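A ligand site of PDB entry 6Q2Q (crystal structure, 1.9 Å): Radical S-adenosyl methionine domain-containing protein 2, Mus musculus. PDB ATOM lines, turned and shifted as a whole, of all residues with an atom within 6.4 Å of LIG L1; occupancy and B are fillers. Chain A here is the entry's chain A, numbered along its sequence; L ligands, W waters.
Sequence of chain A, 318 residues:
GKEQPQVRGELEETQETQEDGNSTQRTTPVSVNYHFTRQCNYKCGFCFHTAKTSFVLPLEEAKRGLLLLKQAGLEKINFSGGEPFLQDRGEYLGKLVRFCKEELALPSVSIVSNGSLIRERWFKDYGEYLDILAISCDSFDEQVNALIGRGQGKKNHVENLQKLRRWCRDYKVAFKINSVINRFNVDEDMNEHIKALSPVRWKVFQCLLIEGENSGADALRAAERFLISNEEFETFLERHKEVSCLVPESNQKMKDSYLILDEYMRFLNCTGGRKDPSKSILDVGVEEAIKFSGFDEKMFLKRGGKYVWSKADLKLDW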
ATOM      1  N   ARG A  38       0.292  20.651   2.057  1.00  0.00           N
ATOM      2  CA  ARG A  38       1.395  20.766   1.113  1.00  0.00           C
ATOM      3  C   ARG A  38       1.974  19.424   0.706  1.00  0.00           C
ATOM      4  O   ARG A  38       2.937  19.395  -0.064  1.00  0.00           O
ATOM      5  CB  ARG A  38       2.486  21.674   1.677  1.00  0.00           C
ATOM      6  CG  ARG A  38       2.102  23.175   1.609  1.00  0.00           C
ATOM      7  CD  ARG A  38       3.191  24.006   2.279  1.00  0.00           C
ATOM      8  NE  ARG A  38       2.961  25.455   2.104  1.00  0.00           N
ATOM      9  CZ  ARG A  38       3.446  26.207   1.119  1.00  0.00           C
ATOM     10  NH1 ARG A  38       4.191  25.677   0.144  1.00  0.00           N
ATOM     11  NH2 ARG A  38       3.160  27.500   1.103  1.00  0.00           N
ATOM     12  N   GLN A  39       1.412  18.317   1.193  1.00  0.00           N
ATOM     13  CA  GLN A  39       1.833  17.005   0.732  1.00  0.00           C
ATOM     14  C   GLN A  39       1.471  16.808  -0.736  1.00  0.00           C
ATOM     15  O   GLN A  39       0.410  17.227  -1.180  1.00  0.00           O
ATOM     16  CB  GLN A  39       1.159  15.909   1.558  1.00  0.00           C
ATOM     17  CG  GLN A  39       1.785  14.542   1.350  1.00  0.00           C
ATOM     18  CD  GLN A  39       1.014  13.424   2.036  1.00  0.00           C
ATOM     19  OE1 GLN A  39       0.025  13.653   2.737  1.00  0.00           O
ATOM     20  NE2 GLN A  39       1.431  12.189   1.795  1.00  0.00           N
ATOM     21  N   CYS A  40       2.336  16.117  -1.488  1.00  0.00           N
ATOM     22  CA  CYS A  40       1.944  15.733  -2.846  1.00  0.00           C
ATOM     23  C   CYS A  40       2.641  14.435  -3.218  1.00  0.00           C
ATOM     24  O   CYS A  40       3.671  14.098  -2.658  1.00  0.00           O
ATOM     25  CB  CYS A  40       2.284  16.813  -3.879  1.00  0.00           C
ATOM     26  SG  CYS A  40       1.563  16.361  -5.486  1.00  0.00           S
ATOM     27  N   ASN A  41       2.032  13.698  -4.149  1.00  0.00           N
ATOM     28  CA  ASN A  41       2.590  12.434  -4.622  1.00  0.00           C
ATOM     29  C   ASN A  41       3.249  12.550  -5.999  1.00  0.00           C
ATOM     30  O   ASN A  41       3.834  11.567  -6.460  1.00  0.00           O
ATOM     31  CB  ASN A  41       1.511  11.341  -4.653  1.00  0.00           C
ATOM     32  CG  ASN A  41       0.310  11.700  -5.522  1.00  0.00           C
ATOM     33  OD1 ASN A  41       0.000  12.872  -5.720  1.00  0.00           O
ATOM     34  ND2 ASN A  41      -0.391  10.683  -6.026  1.00  0.00           N
ATOM     35  N   TYR A  42       3.169  13.713  -6.651  1.00  0.00           N
ATOM     36  CA  TYR A  42       3.875  13.974  -7.908  1.00  0.00           C
ATOM     37  C   TYR A  42       5.112  14.825  -7.639  1.00  0.00           C
ATOM     38  O   TYR A  42       5.347  15.286  -6.518  1.00  0.00           O
ATOM     39  CB  TYR A  42       2.966  14.675  -8.917  1.00  0.00           C
ATOM     40  CG  TYR A  42       1.990  13.771  -9.622  1.00  0.00           C
ATOM     41  CD1 TYR A  42       1.868  12.435  -9.268  1.00  0.00           C
ATOM     42  CD2 TYR A  42       1.198  14.254 -10.663  1.00  0.00           C
ATOM     43  CE1 TYR A  42       0.971  11.596  -9.928  1.00  0.00           C
ATOM     44  CE2 TYR A  42       0.308  13.428 -11.330  1.00  0.00           C
ATOM     45  CZ  TYR A  42       0.197  12.104 -10.961  1.00  0.00           C
ATOM     46  OH  TYR A  42      -0.694  11.292 -11.631  1.00  0.00           O
ATOM     47  N   LYS A  43       5.903  15.069  -8.672  1.00  0.00           N
ATOM     48  CA  LYS A  43       7.084  15.898  -8.456  1.00  0.00           C
ATOM     49  C   LYS A  43       7.328  16.813  -9.651  1.00  0.00           C
ATOM     50  O   LYS A  43       8.450  16.941 -10.152  1.00  0.00           O
ATOM     51  CB  LYS A  43       8.304  15.031  -8.139  1.00  0.00           C
ATOM     52  CG  LYS A  43       8.380  13.740  -8.870  1.00  0.00           C
ATOM     53  CD  LYS A  43       9.257  12.771  -8.078  1.00  0.00           C
ATOM     54  CE  LYS A  43       9.336  11.417  -8.735  1.00  0.00           C
ATOM     55  NZ  LYS A  43      10.070  10.412  -7.905  1.00  0.00           N
ATOM     56  N   CYS A  44       6.267  17.477 -10.107  1.00  0.00           N
ATOM     57  CA  CYS A  44       6.370  18.408 -11.227  1.00  0.00           C
ATOM     58  C   CYS A  44       7.509  19.379 -10.980  1.00  0.00           C
ATOM     59  O   CYS A  44       7.605  19.993  -9.915  1.00  0.00           O
ATOM     60  CB  CYS A  44       5.049  19.159 -11.385  1.00  0.00           C
ATOM     61  SG  CYS A  44       3.624  18.055 -11.371  1.00  0.00           S
ATOM     62  N   GLY A  45       8.380  19.518 -11.984  1.00  0.00           N
ATOM     63  CA  GLY A  45       9.609  20.261 -11.775  1.00  0.00           C
ATOM     64  C   GLY A  45       9.415  21.746 -11.540  1.00  0.00           C
ATOM     65  O   GLY A  45      10.313  22.382 -10.973  1.00  0.00           O
ATOM     66  N   PHE A  46       8.287  22.307 -11.979  1.00  0.00           N
ATOM     67  CA  PHE A  46       8.016  23.737 -11.810  1.00  0.00           C
ATOM     68  C   PHE A  46       7.155  24.054 -10.591  1.00  0.00           C
ATOM     69  O   PHE A  46       6.814  25.232 -10.390  1.00  0.00           O
ATOM     70  CB  PHE A  46       7.338  24.296 -13.060  1.00  0.00           C
ATOM     71  CG  PHE A  46       6.155  23.486 -13.517  1.00  0.00           C
ATOM     72  CD1 PHE A  46       5.012  23.380 -12.720  1.00  0.00           C
ATOM     73  CD2 PHE A  46       6.188  22.817 -14.732  1.00  0.00           C
ATOM     74  CE1 PHE A  46       3.909  22.607 -13.126  1.00  0.00           C
ATOM     75  CE2 PHE A  46       5.092  22.058 -15.146  1.00  0.00           C
ATOM     76  CZ  PHE A  46       3.962  21.946 -14.347  1.00  0.00           C
ATOM     77  N   CYS A  47       6.759  23.047  -9.798  1.00  0.00           N
ATOM     78  CA  CYS A  47       5.721  23.227  -8.783  1.00  0.00           C
ATOM     79  C   CYS A  47       5.931  24.495  -7.940  1.00  0.00           C
ATOM     80  O   CYS A  47       6.986  24.689  -7.347  1.00  0.00           O
ATOM     81  CB  CYS A  47       5.685  22.007  -7.866  1.00  0.00           C
ATOM     82  SG  CYS A  47       4.445  22.146  -6.597  1.00  0.00           S
ATOM     83  N   PHE A  48       4.921  25.372  -7.905  1.00  0.00           N
ATOM     84  CA  PHE A  48       5.056  26.592  -7.124  1.00  0.00           C
ATOM     85  C   PHE A  48       4.330  26.526  -5.769  1.00  0.00           C
ATOM     86  O   PHE A  48       4.191  27.572  -5.114  1.00  0.00           O
ATOM     87  CB  PHE A  48       4.631  27.852  -7.938  1.00  0.00           C
ATOM     88  CG  PHE A  48       3.173  27.925  -8.362  1.00  0.00           C
ATOM     89  CD1 PHE A  48       2.772  28.951  -9.223  1.00  0.00           C
ATOM     90  CD2 PHE A  48       2.206  27.014  -7.932  1.00  0.00           C
ATOM     91  CE1 PHE A  48       1.463  29.093  -9.638  1.00  0.00           C
ATOM     92  CE2 PHE A  48       0.855  27.144  -8.359  1.00  0.00           C
ATOM     93  CZ  PHE A  48       0.494  28.173  -9.212  1.00  0.00           C
ATOM     94  N   HIS A  49       3.904  25.339  -5.318  1.00  0.00           N
ATOM     95  CA  HIS A  49       3.328  25.185  -3.973  1.00  0.00           C
ATOM     96  C   HIS A  49       3.825  23.859  -3.382  1.00  0.00           C
ATOM     97  O   HIS A  49       3.134  22.835  -3.397  1.00  0.00           O
ATOM     98  CB  HIS A  49       1.797  25.266  -3.989  1.00  0.00           C
ATOM     99  CG  HIS A  49       1.224  25.658  -2.669  1.00  0.00           C
ATOM    100  ND1 HIS A  49       0.987  26.976  -2.330  1.00  0.00           N
ATOM    101  CD2 HIS A  49       0.920  24.926  -1.579  1.00  0.00           C
ATOM    102  CE1 HIS A  49       0.522  27.028  -1.098  1.00  0.00           C
ATOM    103  NE2 HIS A  49       0.458  25.795  -0.620  1.00  0.00           N
ATOM    104  N   THR A  50       5.037  23.913  -2.840  1.00  0.00           N
ATOM    105  CA  THR A  50       5.872  22.753  -2.566  1.00  0.00           C
ATOM    106  C   THR A  50       5.651  22.223  -1.146  1.00  0.00           C
ATOM    107  O   THR A  50       4.998  22.855  -0.323  1.00  0.00           O
ATOM    108  CB  THR A  50       7.338  23.133  -2.775  1.00  0.00           C
ATOM    109  OG1 THR A  50       7.687  24.194  -1.888  1.00  0.00           O
ATOM    110  CG2 THR A  50       7.564  23.615  -4.220  1.00  0.00           C
ATOM    111  N   GLY A  81      -3.605  22.408  -3.052  1.00  0.00           N
ATOM    112  CA  GLY A  81      -2.471  22.005  -2.232  1.00  0.00           C
ATOM    113  C   GLY A  81      -1.175  22.298  -2.951  1.00  0.00           C
ATOM    114  O   GLY A  81      -1.062  23.365  -3.560  1.00  0.00           O
ATOM    115  N   GLY A  82      -0.211  21.381  -2.922  1.00  0.00           N
ATOM    116  CA  GLY A  82      -0.370  20.023  -2.430  1.00  0.00           C
ATOM    117  C   GLY A  82      -1.337  19.258  -3.294  1.00  0.00           C
ATOM    118  O   GLY A  82      -1.929  19.821  -4.224  1.00  0.00           O
ATOM    119  N   GLU A  83      -1.542  17.978  -2.990  1.00  0.00           N
ATOM    120  CA  GLU A  83      -2.568  17.191  -3.676  1.00  0.00           C
ATOM    121  C   GLU A  83      -3.730  16.974  -2.720  1.00  0.00           C
ATOM    122  O   GLU A  83      -3.584  16.205  -1.752  1.00  0.00           O
ATOM    123  CB  GLU A  83      -2.012  15.852  -4.163  1.00  0.00           C
ATOM    124  CG  GLU A  83      -3.082  14.908  -4.765  1.00  0.00           C
ATOM    125  CD  GLU A  83      -4.064  15.625  -5.683  1.00  0.00           C
ATOM    126  OE1 GLU A  83      -3.592  16.423  -6.519  1.00  0.00           O
ATOM    127  OE2 GLU A  83      -5.295  15.392  -5.589  1.00  0.00           O
ATOM    128  N   SER A 113      -6.884  19.336  -8.696  1.00  0.00           N
ATOM    129  CA  SER A 113      -6.252  18.083  -8.300  1.00  0.00           C
ATOM    130  C   SER A 113      -5.408  17.530  -9.439  1.00  0.00           C
ATOM    131  O   SER A 113      -5.706  17.750 -10.614  1.00  0.00           O
ATOM    132  CB  SER A 113      -7.301  17.024  -7.892  1.00  0.00           C
ATOM    133  OG  SER A 113      -6.695  15.723  -7.866  1.00  0.00           O
ATOM    134  N   ASN A 114      -4.381  16.750  -9.103  1.00  0.00           N
ATOM    135  CA  ASN A 114      -3.640  16.091 -10.168  1.00  0.00           C
ATOM    136  C   ASN A 114      -4.353  14.846 -10.682  1.00  0.00           C
ATOM    137  O   ASN A 114      -3.874  14.245 -11.644  1.00  0.00           O
ATOM    138  CB  ASN A 114      -2.201  15.766  -9.726  1.00  0.00           C
ATOM    139  CG  ASN A 114      -2.129  14.709  -8.629  1.00  0.00           C
ATOM    140  OD1 ASN A 114      -3.020  13.861  -8.491  1.00  0.00           O
ATOM    141  ND2 ASN A 114      -1.026  14.718  -7.873  1.00  0.00           N
ATOM    142  N   SER A 136      -5.384  18.819 -13.383  1.00  0.00           N
ATOM    143  CA  SER A 136      -4.226  19.404 -14.058  1.00  0.00           C
ATOM    144  C   SER A 136      -3.710  18.430 -15.108  1.00  0.00           C
ATOM    145  O   SER A 136      -3.467  17.256 -14.807  1.00  0.00           O
ATOM    146  CB  SER A 136      -3.130  19.742 -13.060  1.00  0.00           C
ATOM    147  OG  SER A 136      -3.580  20.798 -12.242  1.00  0.00           O
ATOM    148  N   GLY A 149       7.540  15.501 -14.700  1.00  0.00           N
ATOM    149  CA  GLY A 149       7.406  14.892 -13.398  1.00  0.00           C
ATOM    150  C   GLY A 149       5.981  14.638 -12.959  1.00  0.00           C
ATOM    151  O   GLY A 149       5.768  14.421 -11.761  1.00  0.00           O
ATOM    152  N   ARG A 150       5.015  14.637 -13.878  1.00  0.00           N
ATOM    153  CA  ARG A 150       3.625  14.345 -13.553  1.00  0.00           C
ATOM    154  C   ARG A 150       3.445  12.835 -13.509  1.00  0.00           C
ATOM    155  O   ARG A 150       3.158  12.197 -14.501  1.00  0.00           O
ATOM    156  CB  ARG A 150       2.667  14.940 -14.572  1.00  0.00           C
ATOM    157  CG  ARG A 150       2.483  16.399 -14.455  1.00  0.00           C
ATOM    158  CD  ARG A 150       1.127  16.814 -13.867  1.00  0.00           C
ATOM    159  NE  ARG A 150       1.090  18.277 -13.935  1.00  0.00           N
ATOM    160  CZ  ARG A 150       0.554  19.075 -13.015  1.00  0.00           C
ATOM    161  NH1 ARG A 150      -0.024  18.577 -11.944  1.00  0.00           N
ATOM    162  NH2 ARG A 150       0.613  20.385 -13.178  1.00  0.00           N
ATOM    163  N   ARG A 221      12.146  23.318  -5.416  1.00  0.00           N
ATOM    164  CA  ARG A 221      12.162  23.142  -6.859  1.00  0.00           C
ATOM    165  C   ARG A 221      12.973  24.270  -7.479  1.00  0.00           C
ATOM    166  O   ARG A 221      13.306  25.256  -6.826  1.00  0.00           O
ATOM    167  CB  ARG A 221      10.742  23.103  -7.439  1.00  0.00           C
ATOM    168  CG  ARG A 221       9.883  21.952  -6.876  1.00  0.00           C
ATOM    169  CD  ARG A 221      10.481  20.577  -7.209  1.00  0.00           C
ATOM    170  NE  ARG A 221       9.694  19.459  -6.649  1.00  0.00           N
ATOM    171  CZ  ARG A 221      10.180  18.531  -5.831  1.00  0.00           C
ATOM    172  NH1 ARG A 221      11.461  18.569  -5.446  1.00  0.00           N
ATOM    173  NH2 ARG A 221       9.399  17.559  -5.397  1.00  0.00           N
HETATM  174 FE1  LIG L   1       1.989  18.165  -6.878  1.00  0.00          FE
HETATM  175 FE2  LIG L   1       2.594  18.819  -9.374  1.00  0.00          FE
HETATM  176 FE3  LIG L   1       2.918  20.587  -7.423  1.00  0.00          FE
HETATM  177 FE4  LIG L   1       0.346  19.708  -8.149  1.00  0.00          FE
HETATM  178  S1  LIG L   1       1.870  20.953  -9.407  1.00  0.00           S
HETATM  179  S2  LIG L   1       1.235  20.061  -5.990  1.00  0.00           S
HETATM  180  S3  LIG L   1       0.805  17.577  -8.778  1.00  0.00           S
HETATM  181  S4  LIG L   1       4.089  18.705  -7.610  1.00  0.00           S
HETATM  182  N1  LG2 L   2      -1.729  19.192  -6.928  1.00  0.00           N
HETATM  183  C1  LG2 L   2      -2.864  19.870  -7.588  1.00  0.00           C
HETATM  184  C2  LG2 L   2      -3.078  21.290  -7.027  1.00  0.00           C
HETATM  185  C3  LG2 L   2      -1.770  21.984  -6.600  1.00  0.00           C
HETATM  186  S1  LG2 L   2      -1.106  23.077  -7.894  1.00  0.00           S
HETATM  187  C4  LG2 L   2      -2.638  19.949  -9.081  1.00  0.00           C
HETATM  188  O1  LG2 L   2      -1.558  19.743  -9.572  1.00  0.00           O
HETATM  189  O2  LG2 L   2      -3.660  20.223  -9.893  1.00  0.00           O
HETATM  190  C5  LG2 L   2      -2.542  24.114  -8.361  1.00  0.00           C
HETATM  191  C6  LG2 L   2      -2.445  24.491  -9.852  1.00  0.00           C
HETATM  192  O3  LG2 L   2      -1.251  25.297 -10.063  1.00  0.00           O
HETATM  193  C7  LG2 L   2      -2.323  23.265 -10.790  1.00  0.00           C
HETATM  194  O4  LG2 L   2      -3.173  23.426 -11.925  1.00  0.00           O
HETATM  195  C8  LG2 L   2      -0.830  23.299 -11.222  1.00  0.00           C
HETATM  196  O5  LG2 L   2      -0.634  22.712 -12.507  1.00  0.00           O
HETATM  197  C9  LG2 L   2      -0.571  24.822 -11.232  1.00  0.00           C
HETATM  198  N2  LG2 L   2       0.867  25.147 -11.128  1.00  0.00           N
HETATM  199  C10 LG2 L   2       1.824  24.488 -10.398  1.00  0.00           C
HETATM  200  N3  LG2 L   2       2.983  25.083 -10.541  1.00  0.00           N
HETATM  201  C11 LG2 L   2       2.801  26.138 -11.391  1.00  0.00           C
HETATM  202  C12 LG2 L   2       3.662  27.111 -11.908  1.00  0.00           C
HETATM  203  N4  LG2 L   2       5.022  27.101 -11.560  1.00  0.00           N
HETATM  204  N5  LG2 L   2       3.143  28.034 -12.739  1.00  0.00           N
HETATM  205  C13 LG2 L   2       1.855  28.038 -13.063  1.00  0.00           C
HETATM  206  N6  LG2 L   2       1.001  27.140 -12.603  1.00  0.00           N
HETATM  207  C14 LG2 L   2       1.455  26.201 -11.762  1.00  0.00           C
HETATM  208  O   HOH W   1       7.123  18.853  -7.191  1.00  0.00           O
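Residues that only touch LIG L1: Tyr 42 (3.6 Å). Hydrophobic or aromatic side chains that line LIG L1: Tyr 42. Of the 22 residues printed, 7 come within 4 Å of LIG L1. The nearest printed residue that does not touch LIG L1 is Lys 43 (4.2 Å).
The side-chain amide nitrogen (ND2) of Asn 114 sits at hydrogen-bond distance from the side-chain amide oxygen (OD1) of Asn 41. The side-chain sulfur (SG) of Cys 44 sits close to the guanidinium group (NE) of Arg 150, 3.6 Å away. The side-chain carboxylate (OE1) of Glu 83 lies within hydrogen-bond range of the backbone NH (N) of Asn 114, 2.7 Å away. The side-chain sulfur of Cys 47 lies close to the backbone NH of His 49 (3.5 Å). The backbone NH of Tyr 42 sits close to the side-chain sulfur of Cys 40 (3.3 Å).
FE4 of LIG L1 is bound by O1 of LG2 L2, 2.4 Å away.
Water W1 lies within hydrogen-bond range of the guanidinium group of Arg 221 (2.7 Å), the backbone carbonyl oxygen of Cys 44 (3.0 Å) and a sulfur (S4) of LIG L1 (3.1 Å).
S3 of LIG L1 lies close to NH1 of Arg 150. N1 of LG2 L2 lies close to OE1 of Glu 83 (3.4 Å). N of Phe 48 is in hydrogen-bond range of N3 of LG2 L2. A nitrogen (N1) of LG2 L2 sits close to the backbone carbonyl oxygen (O) of Gly 82, at 2.8 Å. SG of Cys 40 is bound to FE1 of LIG L1 (2.3 Å). The side-chain amide nitrogen of Asn 114 lies close to a sulfur (S3) of LIG L1, 3.5 Å away. The backbone NH (N) of Gly 82 lies close to a sulfur (S2) of LIG L1, 3.6 Å away. O2 of LG2 L2 sits at hydrogen-bond distance from OG of Ser 136, at 2.4 Å. A sulfur (S4) of LIG L1 lies close to the backbone NH (N) of Cys 44, at 3.5 Å. The guanidinium group (NH2) of Arg 150 sits at hydrogen-bond distance from an oxygen (O5) of LG2 L2, at 2.7 Å. SG of Cys 47 is bound to FE3 of LIG L1, at 2.3 Å. SG of Cys 44 binds FE2 of LIG L1 (2.4 Å). A nitrogen (N4) of LG2 L2 is in hydrogen-bond range of the backbone carbonyl oxygen (O) of Phe 46, 2.8 Å away.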
